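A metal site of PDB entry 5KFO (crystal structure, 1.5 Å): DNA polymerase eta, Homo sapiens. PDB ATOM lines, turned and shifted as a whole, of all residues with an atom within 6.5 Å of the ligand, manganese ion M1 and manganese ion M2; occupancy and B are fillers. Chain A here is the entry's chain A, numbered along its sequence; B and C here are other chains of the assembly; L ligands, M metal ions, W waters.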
ATOM      1  N   ASP A  16       8.925  -1.570  -9.157  1.00  0.00           N
ATOM      2  CA  ASP A  16       7.990  -2.670  -9.424  1.00  0.00           C
ATOM      3  C   ASP A  16       6.704  -2.470  -8.632  1.00  0.00           C
ATOM      4  O   ASP A  16       6.751  -2.348  -7.414  1.00  0.00           O
ATOM      5  CB  ASP A  16       8.630  -4.002  -9.063  1.00  0.00           C
ATOM      6  CG  ASP A  16       7.750  -5.158  -9.394  1.00  0.00           C
ATOM      7  OD1 ASP A  16       6.859  -5.457  -8.594  1.00  0.00           O
ATOM      8  OD2 ASP A  16       7.952  -5.758 -10.472  1.00  0.00           O
ATOM      9  N   MET A  17       5.553  -2.459  -9.302  1.00  0.00           N
ATOM     10  CA  MET A  17       4.304  -2.195  -8.606  1.00  0.00           C
ATOM     11  C   MET A  17       3.947  -3.287  -7.607  1.00  0.00           C
ATOM     12  O   MET A  17       4.223  -4.452  -7.855  1.00  0.00           O
ATOM     13  CB  MET A  17       3.161  -2.021  -9.617  1.00  0.00           C
ATOM     14  CG  MET A  17       3.454  -1.034 -10.722  1.00  0.00           C
ATOM     15  SD  MET A  17       3.902   0.617 -10.142  1.00  0.00           S
ATOM     16  CE  MET A  17       2.440   1.101  -9.277  1.00  0.00           C
ATOM     17  N   ASP A  18       3.343  -2.922  -6.488  1.00  0.00           N
ATOM     18  CA  ASP A  18       2.914  -3.935  -5.504  1.00  0.00           C
ATOM     19  C   ASP A  18       1.613  -4.563  -5.969  1.00  0.00           C
ATOM     20  O   ASP A  18       0.719  -3.839  -6.406  1.00  0.00           O
ATOM     21  CB  ASP A  18       2.749  -3.307  -4.123  1.00  0.00           C
ATOM     22  CG  ASP A  18       4.043  -2.716  -3.571  1.00  0.00           C
ATOM     23  OD1 ASP A  18       5.143  -3.198  -3.925  1.00  0.00           O
ATOM     24  OD2 ASP A  18       3.945  -1.772  -2.774  1.00  0.00           O
ATOM     25  N   CYS A  19       1.558  -5.892  -5.885  1.00  0.00           N
ATOM     26  CA  CYS A  19       0.395  -6.689  -6.292  1.00  0.00           C
ATOM     27  C   CYS A  19      -0.432  -5.970  -7.362  1.00  0.00           C
ATOM     28  O   CYS A  19      -1.593  -5.611  -7.141  1.00  0.00           O
ATOM     29  CB  CYS A  19      -0.466  -7.068  -5.058  1.00  0.00           C
ATOM     30  SG  CYS A  19      -1.025  -5.771  -3.940  1.00  0.00           S
ATOM     31  N   PHE A  20       0.178  -5.742  -8.515  1.00  0.00           N
ATOM     32  CA  PHE A  20      -0.301  -4.733  -9.456  1.00  0.00           C
ATOM     33  C   PHE A  20      -1.755  -4.887  -9.909  1.00  0.00           C
ATOM     34  O   PHE A  20      -2.528  -3.945  -9.765  1.00  0.00           O
ATOM     35  CB  PHE A  20       0.592  -4.704 -10.704  1.00  0.00           C
ATOM     36  CG  PHE A  20       0.261  -3.584 -11.649  1.00  0.00           C
ATOM     37  CD1 PHE A  20       0.001  -2.313 -11.144  1.00  0.00           C
ATOM     38  CD2 PHE A  20       0.207  -3.787 -13.019  1.00  0.00           C
ATOM     39  CE1 PHE A  20      -0.312  -1.246 -12.009  1.00  0.00           C
ATOM     40  CE2 PHE A  20      -0.107  -2.719 -13.898  1.00  0.00           C
ATOM     41  CZ  PHE A  20      -0.360  -1.465 -13.378  1.00  0.00           C
ATOM     42  N   PHE A  21      -2.118  -6.037 -10.452  1.00  0.00           N
ATOM     43  CA  PHE A  21      -3.485  -6.139 -10.974  1.00  0.00           C
ATOM     44  C   PHE A  21      -4.508  -5.960  -9.844  1.00  0.00           C
ATOM     45  O   PHE A  21      -5.615  -5.449 -10.057  1.00  0.00           O
ATOM     46  CB  PHE A  21      -3.742  -7.484 -11.675  1.00  0.00           C
ATOM     47  CG  PHE A  21      -3.035  -7.656 -13.005  1.00  0.00           C
ATOM     48  CD1 PHE A  21      -2.014  -6.805 -13.417  1.00  0.00           C
ATOM     49  CD2 PHE A  21      -3.394  -8.697 -13.829  1.00  0.00           C
ATOM     50  CE1 PHE A  21      -1.367  -7.013 -14.659  1.00  0.00           C
ATOM     51  CE2 PHE A  21      -2.766  -8.899 -15.056  1.00  0.00           C
ATOM     52  CZ  PHE A  21      -1.749  -8.062 -15.467  1.00  0.00           C
ATOM     53  N   VAL A  22      -4.156  -6.430  -8.639  1.00  0.00           N
ATOM     54  CA  VAL A  22      -5.038  -6.232  -7.487  1.00  0.00           C
ATOM     55  C   VAL A  22      -5.196  -4.737  -7.194  1.00  0.00           C
ATOM     56  O   VAL A  22      -6.315  -4.272  -6.980  1.00  0.00           O
ATOM     57  CB  VAL A  22      -4.493  -6.970  -6.256  1.00  0.00           C
ATOM     58  CG1 VAL A  22      -5.189  -6.472  -4.976  1.00  0.00           C
ATOM     59  CG2 VAL A  22      -4.661  -8.487  -6.414  1.00  0.00           C
ATOM     60  N   GLN A  41      -8.631 -15.295 -13.535  1.00  0.00           N
ATOM     61  CA  GLN A  41      -8.978 -15.429 -14.953  1.00  0.00           C
ATOM     62  C   GLN A  41      -9.879 -16.636 -15.117  1.00  0.00           C
ATOM     63  O   GLN A  41      -9.539 -17.719 -14.649  1.00  0.00           O
ATOM     64  CB  GLN A  41      -7.733 -15.621 -15.815  1.00  0.00           C
ATOM     65  CG  GLN A  41      -7.164 -14.376 -16.418  1.00  0.00           C
ATOM     66  CD  GLN A  41      -5.823 -14.614 -17.084  1.00  0.00           C
ATOM     67  OE1 GLN A  41      -5.168 -15.634 -16.865  1.00  0.00           O
ATOM     68  NE2 GLN A  41      -5.412 -13.675 -17.922  1.00  0.00           N
ATOM     69  N   ILE A  51      -4.080 -14.823 -10.661  1.00  0.00           N
ATOM     70  CA  ILE A  51      -2.871 -14.274 -11.265  1.00  0.00           C
ATOM     71  C   ILE A  51      -2.252 -13.126 -10.464  1.00  0.00           C
ATOM     72  O   ILE A  51      -1.126 -12.711 -10.747  1.00  0.00           O
ATOM     73  CB  ILE A  51      -3.127 -13.810 -12.721  1.00  0.00           C
ATOM     74  CG1 ILE A  51      -4.220 -12.735 -12.791  1.00  0.00           C
ATOM     75  CG2 ILE A  51      -3.463 -15.017 -13.603  1.00  0.00           C
ATOM     76  CD1 ILE A  51      -4.352 -12.135 -14.209  1.00  0.00           C
ATOM     77  N   ALA A  52      -2.954 -12.627  -9.453  1.00  0.00           N
ATOM     78  CA  ALA A  52      -2.397 -11.588  -8.573  1.00  0.00           C
ATOM     79  C   ALA A  52      -3.076 -11.681  -7.210  1.00  0.00           C
ATOM     80  O   ALA A  52      -4.264 -12.038  -7.133  1.00  0.00           O
ATOM     81  CB  ALA A  52      -2.571 -10.177  -9.176  1.00  0.00           C
ATOM     82  N   VAL A  53      -2.321 -11.369  -6.149  1.00  0.00           N
ATOM     83  CA  VAL A  53      -2.755 -11.621  -4.774  1.00  0.00           C
ATOM     84  C   VAL A  53      -2.388 -10.452  -3.864  1.00  0.00           C
ATOM     85  O   VAL A  53      -1.213 -10.076  -3.807  1.00  0.00           O
ATOM     86  CB  VAL A  53      -2.088 -12.912  -4.196  1.00  0.00           C
ATOM     87  CG1 VAL A  53      -2.694 -13.285  -2.845  1.00  0.00           C
ATOM     88  CG2 VAL A  53      -2.255 -14.069  -5.157  1.00  0.00           C
ATOM     89  N   TYR A  55      -1.503  -8.460  -0.363  1.00  0.00           N
ATOM     90  CA  TYR A  55      -0.635  -8.903   0.714  1.00  0.00           C
ATOM     91  C   TYR A  55      -1.416  -9.463   1.889  1.00  0.00           C
ATOM     92  O   TYR A  55      -0.946 -10.405   2.537  1.00  0.00           O
ATOM     93  CB  TYR A  55       0.314  -7.768   1.149  1.00  0.00           C
ATOM     94  CG  TYR A  55       1.466  -7.666   0.185  1.00  0.00           C
ATOM     95  CD1 TYR A  55       1.321  -7.022  -1.036  1.00  0.00           C
ATOM     96  CD2 TYR A  55       2.671  -8.306   0.443  1.00  0.00           C
ATOM     97  CE1 TYR A  55       2.336  -6.965  -1.950  1.00  0.00           C
ATOM     98  CE2 TYR A  55       3.715  -8.258  -0.472  1.00  0.00           C
ATOM     99  CZ  TYR A  55       3.546  -7.590  -1.665  1.00  0.00           C
ATOM    100  OH  TYR A  55       4.570  -7.536  -2.579  1.00  0.00           O
ATOM    101  N   ARG A  58      -1.971 -12.999   0.832  1.00  0.00           N
ATOM    102  CA  ARG A  58      -0.744 -13.795   0.919  1.00  0.00           C
ATOM    103  C   ARG A  58      -0.488 -14.328   2.329  1.00  0.00           C
ATOM    104  O   ARG A  58       0.094 -15.412   2.490  1.00  0.00           O
ATOM    105  CB  ARG A  58       0.462 -12.986   0.460  1.00  0.00           C
ATOM    106  CG  ARG A  58       0.320 -12.494  -0.946  1.00  0.00           C
ATOM    107  CD  ARG A  58       1.563 -11.770  -1.417  1.00  0.00           C
ATOM    108  NE  ARG A  58       1.272 -11.055  -2.664  1.00  0.00           N
ATOM    109  CZ  ARG A  58       2.175 -10.501  -3.454  1.00  0.00           C
ATOM    110  NH1 ARG A  58       3.470 -10.590  -3.154  1.00  0.00           N
ATOM    111  NH2 ARG A  58       1.770  -9.863  -4.565  1.00  0.00           N
ATOM    112  N   ARG A  64      -0.198 -16.914  -6.590  1.00  0.00           N
ATOM    113  CA  ARG A  64      -0.398 -17.041  -8.021  1.00  0.00           C
ATOM    114  C   ARG A  64      -0.404 -18.515  -8.428  1.00  0.00           C
ATOM    115  O   ARG A  64       0.248 -19.334  -7.793  1.00  0.00           O
ATOM    116  CB  ARG A  64       0.691 -16.250  -8.752  1.00  0.00           C
ATOM    117  CG  ARG A  64       0.737 -16.459 -10.239  1.00  0.00           C
ATOM    118  CD  ARG A  64       1.772 -15.542 -10.860  1.00  0.00           C
ATOM    119  NE  ARG A  64       1.455 -14.163 -10.556  1.00  0.00           N
ATOM    120  CZ  ARG A  64       2.249 -13.331  -9.881  1.00  0.00           C
ATOM    121  NH1 ARG A  64       3.444 -13.738  -9.464  1.00  0.00           N
ATOM    122  NH2 ARG A  64       1.837 -12.092  -9.666  1.00  0.00           N
ATOM    123  N   LEU A  92      -6.565  -8.222 -21.234  1.00  0.00           N
ATOM    124  CA  LEU A  92      -5.744  -7.541 -20.214  1.00  0.00           C
ATOM    125  C   LEU A  92      -5.630  -6.036 -20.415  1.00  0.00           C
ATOM    126  O   LEU A  92      -4.770  -5.396 -19.798  1.00  0.00           O
ATOM    127  CB  LEU A  92      -4.343  -8.170 -20.184  1.00  0.00           C
ATOM    128  CG  LEU A  92      -4.306  -9.690 -20.003  1.00  0.00           C
ATOM    129  CD1 LEU A  92      -2.866 -10.212 -20.086  1.00  0.00           C
ATOM    130  CD2 LEU A  92      -4.949 -10.045 -18.658  1.00  0.00           C
ATOM    131  N   SER A 116       8.454  -5.214 -17.757  1.00  0.00           N
ATOM    132  CA  SER A 116       7.243  -6.037 -17.700  1.00  0.00           C
ATOM    133  C   SER A 116       6.037  -5.108 -17.680  1.00  0.00           C
ATOM    134  O   SER A 116       6.183  -3.898 -17.713  1.00  0.00           O
ATOM    135  CB  SER A 116       7.211  -6.931 -16.468  1.00  0.00           C
ATOM    136  OG  SER A 116       6.850  -6.170 -15.312  1.00  0.00           O
ATOM    137  N   ILE A 117       4.840  -5.680 -17.550  1.00  0.00           N
ATOM    138  CA  ILE A 117       3.661  -4.836 -17.464  1.00  0.00           C
ATOM    139  C   ILE A 117       3.680  -3.965 -16.194  1.00  0.00           C
ATOM    140  O   ILE A 117       3.013  -2.940 -16.129  1.00  0.00           O
ATOM    141  CB  ILE A 117       2.376  -5.695 -17.509  1.00  0.00           C
ATOM    142  CG1 ILE A 117       1.159  -4.836 -17.861  1.00  0.00           C
ATOM    143  CG2 ILE A 117       2.163  -6.428 -16.192  1.00  0.00           C
ATOM    144  CD1 ILE A 117      -0.078  -5.681 -18.206  1.00  0.00           C
ATOM    145  N   ASP A 118       4.455  -4.362 -15.179  1.00  0.00           N
ATOM    146  CA  ASP A 118       4.386  -3.607 -13.922  1.00  0.00           C
ATOM    147  C   ASP A 118       5.758  -3.136 -13.388  1.00  0.00           C
ATOM    148  O   ASP A 118       5.860  -2.752 -12.212  1.00  0.00           O
ATOM    149  CB  ASP A 118       3.666  -4.418 -12.829  1.00  0.00           C
ATOM    150  CG  ASP A 118       4.608  -5.258 -11.985  1.00  0.00           C
ATOM    151  OD1 ASP A 118       5.564  -5.899 -12.511  1.00  0.00           O
ATOM    152  OD2 ASP A 118       4.421  -5.191 -10.748  1.00  0.00           O
ATOM    153  N   GLU A 119       6.791  -3.132 -14.222  1.00  0.00           N
ATOM    154  CA  GLU A 119       8.082  -2.648 -13.736  1.00  0.00           C
ATOM    155  C   GLU A 119       8.959  -2.087 -14.809  1.00  0.00           C
ATOM    156  O   GLU A 119       8.850  -2.462 -15.992  1.00  0.00           O
ATOM    157  CB  GLU A 119       8.841  -3.750 -13.000  1.00  0.00           C
ATOM    158  CG  GLU A 119       9.446  -4.805 -13.911  1.00  0.00           C
ATOM    159  CD  GLU A 119       9.528  -6.147 -13.216  1.00  0.00           C
ATOM    160  OE1 GLU A 119      10.610  -6.485 -12.698  1.00  0.00           O
ATOM    161  OE2 GLU A 119       8.500  -6.847 -13.172  1.00  0.00           O
ATOM    162  N   SER A 216       7.291  -0.764  -4.950  1.00  0.00           N
ATOM    163  CA  SER A 216       8.572  -0.901  -4.278  1.00  0.00           C
ATOM    164  C   SER A 216       9.669  -0.592  -5.264  1.00  0.00           C
ATOM    165  O   SER A 216       9.412  -0.474  -6.456  1.00  0.00           O
ATOM    166  CB  SER A 216       8.723  -2.315  -3.724  1.00  0.00           C
ATOM    167  OG  SER A 216       7.706  -2.561  -2.773  1.00  0.00           O
ATOM    168  N   LYS A 227      17.069  -5.071  -9.255  1.00  0.00           N
ATOM    169  CA  LYS A 227      15.936  -5.984  -9.205  1.00  0.00           C
ATOM    170  C   LYS A 227      15.931  -6.794  -7.907  1.00  0.00           C
ATOM    171  O   LYS A 227      14.892  -6.946  -7.242  1.00  0.00           O
ATOM    172  CB  LYS A 227      15.950  -6.928 -10.423  1.00  0.00           C
ATOM    173  CG  LYS A 227      14.838  -7.982 -10.409  1.00  0.00           C
ATOM    174  CD  LYS A 227      13.431  -7.374 -10.445  1.00  0.00           C
ATOM    175  CE  LYS A 227      12.391  -8.491 -10.537  1.00  0.00           C
ATOM    176  NZ  LYS A 227      10.971  -8.007 -10.482  1.00  0.00           N
ATOM    177  N   LYS A 234       9.613  -5.402   0.008  1.00  0.00           N
ATOM    178  CA  LYS A 234       8.222  -5.271  -0.425  1.00  0.00           C
ATOM    179  C   LYS A 234       7.220  -5.586   0.685  1.00  0.00           C
ATOM    180  O   LYS A 234       7.476  -6.455   1.508  1.00  0.00           O
ATOM    181  CB  LYS A 234       7.937  -6.207  -1.610  1.00  0.00           C
ATOM    182  CG  LYS A 234       8.307  -5.678  -2.974  1.00  0.00           C
ATOM    183  CD  LYS A 234       7.661  -6.498  -4.101  1.00  0.00           C
ATOM    184  CE  LYS A 234       7.697  -5.759  -5.454  1.00  0.00           C
ATOM    185  NZ  LYS A 234       6.437  -4.986  -5.730  1.00  0.00           N
ATOM    186  N   PRO A 235       6.068  -4.895   0.699  1.00  0.00           N
ATOM    187  CA  PRO A 235       5.633  -3.877  -0.251  1.00  0.00           C
ATOM    188  C   PRO A 235       5.824  -2.458   0.257  1.00  0.00           C
ATOM    189  O   PRO A 235       6.128  -2.236   1.433  1.00  0.00           O
ATOM    190  CB  PRO A 235       4.136  -4.171  -0.391  1.00  0.00           C
ATOM    191  CG  PRO A 235       3.746  -4.559   1.023  1.00  0.00           C
ATOM    192  CD  PRO A 235       4.971  -5.267   1.616  1.00  0.00           C
ATOM    193  P    DT B   8      11.810 -10.622 -14.009  1.00  0.00           P
ATOM    194  OP1  DT B   8      12.674  -9.467 -14.301  1.00  0.00           O
ATOM    195  OP2  DT B   8      12.001 -11.397 -12.770  1.00  0.00           O
ATOM    196  O5'  DT B   8      10.360 -10.017 -14.057  1.00  0.00           O
ATOM    197  C5'  DT B   8       9.330 -10.842 -13.894  1.00  0.00           C
ATOM    198  C4'  DT B   8       8.073 -10.215 -14.390  1.00  0.00           C
ATOM    199  O4'  DT B   8       7.558 -11.097 -15.406  1.00  0.00           O
ATOM    200  C3'  DT B   8       7.036 -10.151 -13.282  1.00  0.00           C
ATOM    201  O3'  DT B   8       6.389  -8.882 -13.229  1.00  0.00           O
ATOM    202  C2'  DT B   8       6.074 -11.304 -13.588  1.00  0.00           C
ATOM    203  C1'  DT B   8       6.239 -11.497 -15.088  1.00  0.00           C
ATOM    204  N1   DT B   8       6.062 -12.915 -15.498  1.00  0.00           N
ATOM    205  C2   DT B   8       5.062 -13.220 -16.394  1.00  0.00           C
ATOM    206  O2   DT B   8       4.320 -12.372 -16.850  1.00  0.00           O
ATOM    207  N3   DT B   8       4.968 -14.539 -16.727  1.00  0.00           N
ATOM    208  C4   DT B   8       5.740 -15.572 -16.264  1.00  0.00           C
ATOM    209  O4   DT B   8       5.564 -16.744 -16.622  1.00  0.00           O
ATOM    210  C5   DT B   8       6.771 -15.200 -15.330  1.00  0.00           C
ATOM    211  C7   DT B   8       7.683 -16.261 -14.765  1.00  0.00           C
ATOM    212  C6   DT B   8       6.890 -13.903 -14.997  1.00  0.00           C
ATOM    213  P    DT C   3      -2.786 -27.749 -14.105  1.00  0.00           P
ATOM    214  OP1  DT C   3      -1.914 -28.689 -14.855  1.00  0.00           O
ATOM    215  OP2  DT C   3      -3.172 -28.051 -12.709  1.00  0.00           O
ATOM    216  O5'  DT C   3      -2.102 -26.306 -14.134  1.00  0.00           O
ATOM    217  C5'  DT C   3      -2.830 -25.167 -13.690  1.00  0.00           C
ATOM    218  C4'  DT C   3      -2.089 -23.892 -14.053  1.00  0.00           C
ATOM    219  O4'  DT C   3      -0.955 -23.731 -13.170  1.00  0.00           O
ATOM    220  C3'  DT C   3      -1.528 -23.879 -15.472  1.00  0.00           C
ATOM    221  O3'  DT C   3      -2.182 -22.876 -16.256  1.00  0.00           O
ATOM    222  C2'  DT C   3      -0.025 -23.601 -15.317  1.00  0.00           C
ATOM    223  C1'  DT C   3       0.111 -23.160 -13.869  1.00  0.00           C
ATOM    224  N1   DT C   3       1.391 -23.617 -13.247  1.00  0.00           N
ATOM    225  C2   DT C   3       2.302 -22.685 -12.808  1.00  0.00           C
ATOM    226  O2   DT C   3       2.129 -21.489 -12.898  1.00  0.00           O
ATOM    227  N3   DT C   3       3.431 -23.219 -12.248  1.00  0.00           N
ATOM    228  C4   DT C   3       3.739 -24.562 -12.092  1.00  0.00           C
ATOM    229  O4   DT C   3       4.788 -24.943 -11.578  1.00  0.00           O
ATOM    230  C5   DT C   3       2.736 -25.484 -12.570  1.00  0.00           C
ATOM    231  C7   DT C   3       2.953 -26.957 -12.455  1.00  0.00           C
ATOM    232  C6   DT C   3       1.620 -24.975 -13.123  1.00  0.00           C
ATOM    233  P    DT C   4      -4.165 -23.737 -18.611  1.00  0.00           P
ATOM    234  OP1  DT C   4      -5.552 -24.097 -18.972  1.00  0.00           O
ATOM    235  OP2  DT C   4      -3.015 -24.300 -19.347  1.00  0.00           O
ATOM    236  O5'  DT C   4      -4.037 -22.157 -18.717  1.00  0.00           O
ATOM    237  C5'  DT C   4      -4.864 -21.354 -17.927  1.00  0.00           C
ATOM    238  C4'  DT C   4      -4.740 -19.901 -18.345  1.00  0.00           C
ATOM    239  O4'  DT C   4      -3.683 -19.240 -17.624  1.00  0.00           O
ATOM    240  C3'  DT C   4      -4.471 -19.636 -19.813  1.00  0.00           C
ATOM    241  O3'  DT C   4      -5.240 -18.527 -20.223  1.00  0.00           O
ATOM    242  C2'  DT C   4      -2.961 -19.319 -19.837  1.00  0.00           C
ATOM    243  C1'  DT C   4      -2.833 -18.574 -18.531  1.00  0.00           C
ATOM    244  N1   DT C   4      -1.503 -18.573 -17.917  1.00  0.00           N
ATOM    245  C2   DT C   4      -1.129 -17.428 -17.269  1.00  0.00           C
ATOM    246  O2   DT C   4      -1.814 -16.424 -17.266  1.00  0.00           O
ATOM    247  N3   DT C   4       0.085 -17.505 -16.654  1.00  0.00           N
ATOM    248  C4   DT C   4       0.939 -18.577 -16.597  1.00  0.00           C
ATOM    249  O4   DT C   4       2.016 -18.512 -16.012  1.00  0.00           O
ATOM    250  C5   DT C   4       0.467 -19.769 -17.268  1.00  0.00           C
ATOM    251  C7   DT C   4       1.318 -21.022 -17.287  1.00  0.00           C
ATOM    252  C6   DT C   4      -0.732 -19.712 -17.882  1.00  0.00           C
ATOM    253  P    DA C   5      -5.182 -17.980 -21.723  1.00  0.00           P
ATOM    254  OP1  DA C   5      -6.548 -17.558 -22.099  1.00  0.00           O
ATOM    255  OP2  DA C   5      -4.421 -18.936 -22.553  1.00  0.00           O
ATOM    256  O5'  DA C   5      -4.269 -16.692 -21.620  1.00  0.00           O
ATOM    257  C5'  DA C   5      -4.747 -15.545 -20.909  1.00  0.00           C
ATOM    258  C4'  DA C   5      -3.761 -14.411 -21.071  1.00  0.00           C
ATOM    259  O4'  DA C   5      -2.549 -14.715 -20.318  1.00  0.00           O
ATOM    260  C3'  DA C   5      -3.314 -14.145 -22.510  1.00  0.00           C
ATOM    261  O3'  DA C   5      -3.188 -12.740 -22.714  1.00  0.00           O
ATOM    262  C2'  DA C   5      -1.954 -14.834 -22.582  1.00  0.00           C
ATOM    263  C1'  DA C   5      -1.442 -14.564 -21.169  1.00  0.00           C
ATOM    264  N9   DA C   5      -0.405 -15.475 -20.715  1.00  0.00           N
ATOM    265  C8   DA C   5      -0.293 -16.808 -20.999  1.00  0.00           C
ATOM    266  N7   DA C   5       0.730 -17.385 -20.433  1.00  0.00           N
ATOM    267  C5   DA C   5       1.342 -16.358 -19.724  1.00  0.00           C
ATOM    268  C6   DA C   5       2.492 -16.316 -18.914  1.00  0.00           C
ATOM    269  N6   DA C   5       3.259 -17.382 -18.669  1.00  0.00           N
ATOM    270  N1   DA C   5       2.820 -15.140 -18.357  1.00  0.00           N
ATOM    271  C2   DA C   5       2.045 -14.065 -18.610  1.00  0.00           C
ATOM    272  N3   DA C   5       0.947 -13.978 -19.349  1.00  0.00           N
ATOM    273  C4   DA C   5       0.651 -15.184 -19.885  1.00  0.00           C
HETATM  274  P1  LIG L   1       4.481  -8.094  -6.092  1.00  0.00           P
HETATM  275  O1  LIG L   1       5.260  -7.481  -7.142  1.00  0.00           O
HETATM  276  O2  LIG L   1       4.086  -7.076  -5.138  1.00  0.00           O
HETATM  277  O3  LIG L   1       5.070  -9.307  -5.451  1.00  0.00           O
HETATM  278  P2  LIG L   1       2.670  -8.458  -8.299  1.00  0.00           P
HETATM  279  O4  LIG L   1       2.780  -7.080  -8.798  1.00  0.00           O
HETATM  280  O5  LIG L   1       1.284  -8.933  -8.478  1.00  0.00           O
HETATM  281  O6  LIG L   1       3.121  -8.547  -6.768  1.00  0.00           O
HETATM  282  P3  LIG L   1       4.587  -9.315 -10.270  1.00  0.00           P
HETATM  283  S1  LIG L   1       5.644 -10.972 -10.229  1.00  0.00           S
HETATM  284  O7  LIG L   1       5.402  -8.101 -10.279  1.00  0.00           O
HETATM  285  O8  LIG L   1       3.639  -9.497  -9.005  1.00  0.00           O
HETATM  286  O9  LIG L   1       3.688  -9.322 -11.502  1.00  0.00           O
HETATM  287  C1  LIG L   1       3.070  -8.191 -11.926  1.00  0.00           C
HETATM  288  C2  LIG L   1       1.677  -8.445 -12.518  1.00  0.00           C
HETATM  289  O10 LIG L   1       1.839  -9.250 -13.635  1.00  0.00           O
HETATM  290  C3  LIG L   1       0.799  -9.202 -11.655  1.00  0.00           C
HETATM  291  O11 LIG L   1      -0.019  -8.406 -10.830  1.00  0.00           O
HETATM  292  C4  LIG L   1      -0.047  -9.979 -12.550  1.00  0.00           C
HETATM  293  C5  LIG L   1       0.867 -10.281 -13.677  1.00  0.00           C
HETATM  294  N1  LIG L   1       1.513 -11.562 -13.673  1.00  0.00           N
HETATM  295  C6  LIG L   1       2.635 -11.913 -13.049  1.00  0.00           C
HETATM  296  N2  LIG L   1       2.945 -13.146 -13.282  1.00  0.00           N
HETATM  297  C7  LIG L   1       2.060 -13.676 -14.052  1.00  0.00           C
HETATM  298  C8  LIG L   1       1.801 -14.927 -14.672  1.00  0.00           C
HETATM  299  N3  LIG L   1       2.702 -15.960 -14.448  1.00  0.00           N
HETATM  300  N4  LIG L   1       0.719 -15.098 -15.457  1.00  0.00           N
HETATM  301  C9  LIG L   1      -0.180 -14.127 -15.707  1.00  0.00           C
HETATM  302  N5  LIG L   1       0.045 -12.913 -15.140  1.00  0.00           N
HETATM  303  C10 LIG L   1       1.108 -12.668 -14.322  1.00  0.00           C
HETATM  304 MN    MN M   1       7.012  -7.292 -11.655  1.00  0.00          MN
HETATM  305 MN    MN M   2       4.893  -6.193  -8.943  1.00  0.00          MN
HETATM  306  O   HOH W   1       7.887  -8.532  -7.694  1.00  0.00           O
HETATM  307  O   HOH W   2       8.115  -8.755 -10.427  1.00  0.00           O
HETATM  308  O   HOH W   3       4.755 -11.912  -6.559  1.00  0.00           O
HETATM  309  O   HOH W   4       4.425  -8.825 -14.798  1.00  0.00           O
HETATM  310  O   HOH W   5       2.398 -10.431 -16.869  1.00  0.00           O
HETATM  311  O   HOH W   6      -1.547 -11.393 -16.953  1.00  0.00           O
HETATM  312  O   HOH W   7       5.001 -14.889 -12.349  1.00  0.00           O
HETATM  313  O   HOH W   8       0.378 -10.953  -6.877  1.00  0.00           O
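The side-chain hydroxyl (OH) of Tyr 55 sits at hydrogen-bond distance from an oxygen (O2) of the ligand, at 2.6 Å.
A nitrogen (N3) of the ligand lies within hydrogen-bond range of O4 of DT 4 of chain C, 3.1 Å away.
N of Cys 19 sits at hydrogen-bond distance from O2 of the ligand.
An oxygen (O3) of the ligand is in salt-bridge range of the guanidinium group (NH1) of Arg 58, 3.1 Å away.
The backbone NH of Phe 20 sits at hydrogen-bond distance from an oxygen (O5) of the ligand (3.4 Å).
An oxygen (O2) of the ligand lies within salt-bridge range of the side-chain amino group of Lys 234 (3.2 Å).
The backbone NH of Phe 21 is in hydrogen-bond range of an oxygen (O11) of the ligand (3.2 Å).
O5 of the ligand lies within salt-bridge range of NH2 of Arg 64, at 3.4 Å.
OD2 of Asp 16 lies close to NZ of Lys 227 (3.8 Å).
The side-chain amino group of Lys 234 sits close to the backbone carbonyl oxygen of Met 17 (3.1 Å).
The side-chain hydroxyl of Ser 116 sits at hydrogen-bond distance from the backbone NH of Glu 119 (3.2 Å).
The side-chain amino group of Lys 227 lies within salt-bridge range of the side-chain carboxylate of Glu 119, 2.7 Å away.
O2 of DT 4 of chain C sits close to OE1 of Gln 41, 3.5 Å away.
The guanidinium group (NE) of Arg 58 lies within hydrogen-bond range of the backbone carbonyl oxygen (O) of Val 53, at 2.9 Å.
The side-chain amino group (NZ) of Lys 234 lies within salt-bridge range of the side-chain carboxylate (OD1) of Asp 18, 2.9 Å away.
The guanidinium group of Arg 64 sits at hydrogen-bond distance from the backbone carbonyl oxygen of Ile 51, at 3.0 Å.
Merely in contact with the ligand: Asp 18 (3.4 Å), Ile 51 (3.4 Å), Ala 52 (3.5 Å), Ile 117 (3.8 Å) and DA 5 of chain C (3.6 Å).
Hydrophobic or aromatic side chains within 4 Å of the ligand: Phe 20, Phe 21, Ile 51, Ala 52, Tyr 55 and Ile 117.
Of the 27 residues printed, 17 come within 4 Å of the ligand.
The nearest printed residue that does not touch the ligand is Glu 119 (4.4 Å).
Merely in contact with manganese ion M1: Ser 116 (3.8 Å).
Within 4 Å of manganese ion M1: Asp 16, Ser 116, Asp 118, Glu 119 and DT 8 of chain B.
Along chain A the residues within 4 Å of manganese ion M1 span positions 16 to 119.
Merely in contact with manganese ion M2: Lys 234.
Of the 27 residues printed, 4 come within 4 Å of manganese ion M2.
The nearest printed residue that does not touch manganese ion M2 is Asp 18 (4.4 Å).
Manganese ion M1 is bound by the side-chain carboxylate (OD2) of Asp 16, the side-chain carboxylate (OE2) of Glu 119, the side-chain carboxylate (OD1) of Asp 118, water W2, an oxygen (O7) of the ligand and O3' of DT 8 of chain B.
Manganese ion M2 is bound by OD2 of Asp 118 (2.1 Å), OD1 of Asp 16 (2.1 Å), O of Met 17 (2.2 Å), O1 of the ligand (2.2 Å), O4 of the ligand (2.3 Å) and O7 of the ligand (2.4 Å).
Water W2 bridges NZ of Lys 227 (3.0 Å) and S1 of the ligand (3.3 Å).
Water W7 lies within hydrogen-bond range of a nitrogen (N2) of the ligand and the guanidinium group (NH1) of Arg 64.
Water W5 bridges O2 of DT 8 of chain B (2.7 Å) and an oxygen (O10) of the ligand (3.5 Å).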
